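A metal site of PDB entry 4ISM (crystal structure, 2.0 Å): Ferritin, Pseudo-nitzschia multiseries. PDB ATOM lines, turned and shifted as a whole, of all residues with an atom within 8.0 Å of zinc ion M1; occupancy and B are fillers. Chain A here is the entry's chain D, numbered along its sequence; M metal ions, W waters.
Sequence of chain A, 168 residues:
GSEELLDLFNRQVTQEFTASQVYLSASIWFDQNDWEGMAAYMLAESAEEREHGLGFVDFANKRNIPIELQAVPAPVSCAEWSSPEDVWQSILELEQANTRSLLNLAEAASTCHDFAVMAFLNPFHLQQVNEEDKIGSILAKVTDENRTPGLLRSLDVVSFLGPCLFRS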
ATOM      1  N   TYR A  23       7.349  12.099 -11.852  1.00  0.00           N
ATOM      2  CA  TYR A  23       6.643  12.497 -13.143  1.00  0.00           C
ATOM      3  C   TYR A  23       7.582  12.482 -14.307  1.00  0.00           C
ATOM      4  O   TYR A  23       7.195  11.982 -15.327  1.00  0.00           O
ATOM      5  CB  TYR A  23       6.082  13.923 -13.009  1.00  0.00           C
ATOM      6  CG  TYR A  23       4.748  13.903 -12.300  1.00  0.00           C
ATOM      7  CD1 TYR A  23       4.612  14.328 -10.993  1.00  0.00           C
ATOM      8  CD2 TYR A  23       3.583  13.468 -12.979  1.00  0.00           C
ATOM      9  CE1 TYR A  23       3.339  14.377 -10.351  1.00  0.00           C
ATOM     10  CE2 TYR A  23       2.333  13.534 -12.346  1.00  0.00           C
ATOM     11  CZ  TYR A  23       2.221  13.996 -11.051  1.00  0.00           C
ATOM     12  OH  TYR A  23       0.965  14.001 -10.426  1.00  0.00           O
ATOM     13  N   TYR A  41       1.883  15.025 -20.920  1.00  0.00           N
ATOM     14  CA  TYR A  41       1.123  15.326 -19.672  1.00  0.00           C
ATOM     15  C   TYR A  41       2.035  15.124 -18.460  1.00  0.00           C
ATOM     16  O   TYR A  41       2.028  15.941 -17.534  1.00  0.00           O
ATOM     17  CB  TYR A  41      -0.148  14.424 -19.522  1.00  0.00           C
ATOM     18  CG  TYR A  41      -0.921  14.544 -18.183  1.00  0.00           C
ATOM     19  CD1 TYR A  41      -2.082  15.324 -18.070  1.00  0.00           C
ATOM     20  CD2 TYR A  41      -0.479  13.882 -17.031  1.00  0.00           C
ATOM     21  CE1 TYR A  41      -2.804  15.436 -16.861  1.00  0.00           C
ATOM     22  CE2 TYR A  41      -1.155  14.030 -15.828  1.00  0.00           C
ATOM     23  CZ  TYR A  41      -2.318  14.805 -15.757  1.00  0.00           C
ATOM     24  OH  TYR A  41      -2.975  14.922 -14.544  1.00  0.00           O
ATOM     25  N   ALA A  44       4.583  17.982 -18.265  1.00  0.00           N
ATOM     26  CA  ALA A  44       3.954  19.223 -17.746  1.00  0.00           C
ATOM     27  C   ALA A  44       3.814  19.135 -16.237  1.00  0.00           C
ATOM     28  O   ALA A  44       4.169  20.107 -15.542  1.00  0.00           O
ATOM     29  CB  ALA A  44       2.575  19.457 -18.378  1.00  0.00           C
ATOM     30  N   GLU A  45       3.365  17.979 -15.706  1.00  0.00           N
ATOM     31  CA  GLU A  45       3.234  17.798 -14.308  1.00  0.00           C
ATOM     32  C   GLU A  45       4.552  17.791 -13.583  1.00  0.00           C
ATOM     33  O   GLU A  45       4.664  18.250 -12.412  1.00  0.00           O
ATOM     34  CB  GLU A  45       2.482  16.499 -13.948  1.00  0.00           C
ATOM     35  CG  GLU A  45       0.996  16.605 -14.255  1.00  0.00           C
ATOM     36  CD  GLU A  45       0.384  17.629 -13.309  1.00  0.00           C
ATOM     37  OE1 GLU A  45       0.800  17.681 -12.109  1.00  0.00           O
ATOM     38  OE2 GLU A  45      -0.470  18.413 -13.751  1.00  0.00           O
ATOM     39  N   SER A  46       5.560  17.248 -14.241  1.00  0.00           N
ATOM     40  CA  SER A  46       6.926  17.363 -13.659  1.00  0.00           C
ATOM     41  C   SER A  46       7.393  18.866 -13.387  1.00  0.00           C
ATOM     42  O   SER A  46       7.952  19.215 -12.317  1.00  0.00           O
ATOM     43  CB  SER A  46       7.938  16.573 -14.554  1.00  0.00           C
ATOM     44  OG  SER A  46       9.271  16.726 -14.025  1.00  0.00           O
ATOM     45  N   GLU A  48       5.419  21.407 -13.049  1.00  0.00           N
ATOM     46  CA  GLU A  48       4.560  21.954 -12.036  1.00  0.00           C
ATOM     47  C   GLU A  48       4.979  21.565 -10.613  1.00  0.00           C
ATOM     48  O   GLU A  48       4.840  22.405  -9.676  1.00  0.00           O
ATOM     49  CB  GLU A  48       3.147  21.436 -12.268  1.00  0.00           C
ATOM     50  CG  GLU A  48       2.161  21.811 -11.174  1.00  0.00           C
ATOM     51  CD  GLU A  48       0.825  21.132 -11.443  1.00  0.00           C
ATOM     52  OE1 GLU A  48       0.304  21.236 -12.590  1.00  0.00           O
ATOM     53  OE2 GLU A  48       0.332  20.435 -10.530  1.00  0.00           O
ATOM     54  N   GLU A  49       5.377  20.311 -10.408  1.00  0.00           N
ATOM     55  CA  GLU A  49       5.822  19.922  -9.057  1.00  0.00           C
ATOM     56  C   GLU A  49       7.049  20.700  -8.715  1.00  0.00           C
ATOM     57  O   GLU A  49       7.288  21.070  -7.519  1.00  0.00           O
ATOM     58  CB  GLU A  49       6.162  18.405  -8.993  1.00  0.00           C
ATOM     59  CG  GLU A  49       4.953  17.505  -9.145  1.00  0.00           C
ATOM     60  CD  GLU A  49       3.923  17.713  -8.046  1.00  0.00           C
ATOM     61  OE1 GLU A  49       4.276  18.220  -6.990  1.00  0.00           O
ATOM     62  OE2 GLU A  49       2.715  17.475  -8.238  1.00  0.00           O
ATOM     63  N   HIS A  52       5.963  23.977  -7.476  1.00  0.00           N
ATOM     64  CA  HIS A  52       5.490  23.857  -6.062  1.00  0.00           C
ATOM     65  C   HIS A  52       6.672  23.890  -5.072  1.00  0.00           C
ATOM     66  O   HIS A  52       6.598  24.552  -4.042  1.00  0.00           O
ATOM     67  CB  HIS A  52       4.746  22.511  -5.755  1.00  0.00           C
ATOM     68  CG  HIS A  52       3.465  22.309  -6.516  1.00  0.00           C
ATOM     69  ND1 HIS A  52       2.860  21.081  -6.597  1.00  0.00           N
ATOM     70  CD2 HIS A  52       2.692  23.155  -7.252  1.00  0.00           C
ATOM     71  CE1 HIS A  52       1.789  21.162  -7.369  1.00  0.00           C
ATOM     72  NE2 HIS A  52       1.667  22.409  -7.798  1.00  0.00           N
ATOM     73  N   GLU A  95       0.706  11.234  -5.567  1.00  0.00           N
ATOM     74  CA  GLU A  95      -0.081  12.410  -5.127  1.00  0.00           C
ATOM     75  C   GLU A  95      -0.728  12.196  -3.788  1.00  0.00           C
ATOM     76  O   GLU A  95      -0.822  13.118  -2.990  1.00  0.00           O
ATOM     77  CB  GLU A  95      -1.142  12.768  -6.135  1.00  0.00           C
ATOM     78  CG  GLU A  95      -0.604  13.384  -7.389  1.00  0.00           C
ATOM     79  CD  GLU A  95       0.134  14.697  -7.160  1.00  0.00           C
ATOM     80  OE1 GLU A  95       0.039  15.336  -6.076  1.00  0.00           O
ATOM     81  OE2 GLU A  95       0.783  15.101  -8.134  1.00  0.00           O
ATOM     82  N   GLN A 127      -5.278  22.447  -4.162  1.00  0.00           N
ATOM     83  CA  GLN A 127      -4.663  21.877  -5.397  1.00  0.00           C
ATOM     84  C   GLN A 127      -4.651  20.348  -5.332  1.00  0.00           C
ATOM     85  O   GLN A 127      -5.043  19.691  -6.314  1.00  0.00           O
ATOM     86  CB  GLN A 127      -3.231  22.403  -5.629  1.00  0.00           C
ATOM     87  CG  GLN A 127      -2.383  21.550  -6.582  1.00  0.00           C
ATOM     88  CD  GLN A 127      -2.613  21.921  -8.019  1.00  0.00           C
ATOM     89  OE1 GLN A 127      -3.479  22.734  -8.300  1.00  0.00           O
ATOM     90  NE2 GLN A 127      -1.832  21.329  -8.946  1.00  0.00           N
ATOM     91  N   GLN A 128      -4.200  19.794  -4.206  1.00  0.00           N
ATOM     92  CA  GLN A 128      -4.136  18.315  -4.006  1.00  0.00           C
ATOM     93  C   GLN A 128      -5.468  17.645  -4.190  1.00  0.00           C
ATOM     94  O   GLN A 128      -5.557  16.603  -4.847  1.00  0.00           O
ATOM     95  CB  GLN A 128      -3.607  17.948  -2.583  1.00  0.00           C
ATOM     96  CG  GLN A 128      -2.132  18.154  -2.371  1.00  0.00           C
ATOM     97  CD  GLN A 128      -1.307  17.499  -3.479  1.00  0.00           C
ATOM     98  OE1 GLN A 128      -0.719  18.179  -4.287  1.00  0.00           O
ATOM     99  NE2 GLN A 128      -1.375  16.163  -3.565  1.00  0.00           N
ATOM    100  N   ASN A 130      -7.835  18.651  -6.238  1.00  0.00           N
ATOM    101  CA  ASN A 130      -8.043  18.646  -7.680  1.00  0.00           C
ATOM    102  C   ASN A 130      -7.128  17.660  -8.409  1.00  0.00           C
ATOM    103  O   ASN A 130      -7.594  16.964  -9.341  1.00  0.00           O
ATOM    104  CB  ASN A 130      -7.838  20.029  -8.259  1.00  0.00           C
ATOM    105  CG  ASN A 130      -8.910  21.038  -7.818  1.00  0.00           C
ATOM    106  OD1 ASN A 130      -9.995  20.704  -7.301  1.00  0.00           O
ATOM    107  ND2 ASN A 130      -8.627  22.296  -8.096  1.00  0.00           N
ATOM    108  N   GLU A 131      -5.877  17.576  -7.979  1.00  0.00           N
ATOM    109  CA  GLU A 131      -4.932  16.666  -8.639  1.00  0.00           C
ATOM    110  C   GLU A 131      -5.333  15.220  -8.421  1.00  0.00           C
ATOM    111  O   GLU A 131      -5.355  14.413  -9.376  1.00  0.00           O
ATOM    112  CB  GLU A 131      -3.505  16.839  -8.123  1.00  0.00           C
ATOM    113  CG  GLU A 131      -2.520  16.263  -9.110  1.00  0.00           C
ATOM    114  CD  GLU A 131      -2.282  17.219 -10.266  1.00  0.00           C
ATOM    115  OE1 GLU A 131      -1.864  18.344  -9.981  1.00  0.00           O
ATOM    116  OE2 GLU A 131      -2.540  16.863 -11.441  1.00  0.00           O
ATOM    117  N   GLU A 132      -5.626  14.875  -7.170  1.00  0.00           N
ATOM    118  CA  GLU A 132      -6.072  13.460  -6.890  1.00  0.00           C
ATOM    119  C   GLU A 132      -7.323  13.059  -7.696  1.00  0.00           C
ATOM    120  O   GLU A 132      -7.444  11.934  -8.215  1.00  0.00           O
ATOM    121  CB  GLU A 132      -6.300  13.193  -5.429  1.00  0.00           C
ATOM    122  CG  GLU A 132      -5.007  13.117  -4.618  1.00  0.00           C
ATOM    123  CD  GLU A 132      -5.268  12.658  -3.178  1.00  0.00           C
ATOM    124  OE1 GLU A 132      -6.096  11.747  -2.933  1.00  0.00           O
ATOM    125  OE2 GLU A 132      -4.659  13.217  -2.267  1.00  0.00           O
ATOM    126  N   LYS A 134      -8.286  14.447 -10.594  1.00  0.00           N
ATOM    127  CA  LYS A 134      -8.050  14.323 -12.029  1.00  0.00           C
ATOM    128  C   LYS A 134      -7.287  12.983 -12.322  1.00  0.00           C
ATOM    129  O   LYS A 134      -7.596  12.220 -13.290  1.00  0.00           O
ATOM    130  CB  LYS A 134      -7.221  15.563 -12.500  1.00  0.00           C
ATOM    131  CG  LYS A 134      -6.796  15.507 -13.993  1.00  0.00           C
ATOM    132  CD  LYS A 134      -5.821  16.603 -14.371  1.00  0.00           C
ATOM    133  CE  LYS A 134      -4.735  16.797 -13.279  1.00  0.00           C
ATOM    134  NZ  LYS A 134      -3.735  17.885 -13.522  1.00  0.00           N
ATOM    135  N   ILE A 135      -6.314  12.646 -11.470  1.00  0.00           N
ATOM    136  CA  ILE A 135      -5.497  11.434 -11.751  1.00  0.00           C
ATOM    137  C   ILE A 135      -6.373  10.247 -11.582  1.00  0.00           C
ATOM    138  O   ILE A 135      -6.288   9.297 -12.370  1.00  0.00           O
ATOM    139  CB  ILE A 135      -4.240  11.303 -10.826  1.00  0.00           C
ATOM    140  CG1 ILE A 135      -3.233  12.315 -11.296  1.00  0.00           C
ATOM    141  CG2 ILE A 135      -3.565   9.916 -10.876  1.00  0.00           C
ATOM    142  CD1 ILE A 135      -2.433  12.766 -10.119  1.00  0.00           C
HETATM  143 ZN    ZN M   1      -1.171  19.351 -11.881  1.00  0.00          ZN
HETATM  144 ZN    ZN M   2       1.265  17.162  -7.252  1.00  0.00          ZN
HETATM  145 ZN    ZN M   3       3.179  19.332  -5.519  1.00  0.00          ZN
HETATM  146  O   HOH W   1      -2.736  20.220 -12.584  1.00  0.00           O
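OE2 of Glu 45 sits close to NZ of Lys 134, 3.3 Å away.
The side-chain amino group (NZ) of Lys 134 is in salt-bridge range of the side-chain carboxylate (OE2) of Glu 131.
NE2 of Gln 127 sits close to OE1 of Glu 131 (3.2 Å).
The side-chain amide nitrogen (NE2) of Gln 127 sits close to the side-chain carboxylate (OE2) of Glu 48 (2.8 Å).
The side-chain amino group of Lys 134 lies close to the side-chain hydroxyl of Tyr 41, 3.2 Å away.
Merely in contact with zinc ion M1: Gln 127 (3.6 Å) and Lys 134 (3.4 Å).
Of the 16 residues printed, 5 come within 4 Å of zinc ion M1.
The nearest printed residue that does not touch zinc ion M1 is Tyr 41 (5.5 Å).
Zinc ion M1 is bound by water W1 (1.9 Å), the side-chain carboxylate (OE2) of Glu 45 (2.2 Å), the side-chain carboxylate (OE1) of Glu 131 (2.3 Å), the side-chain carboxylate (OE2) of Glu 48 (2.3 Å), the side-chain carboxylate (OE1) of Glu 48 (2.5 Å) and the side-chain carboxylate (OE1) of Glu 45 (2.6 Å).
Zinc ion M1 has six donor atoms within binding distance.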
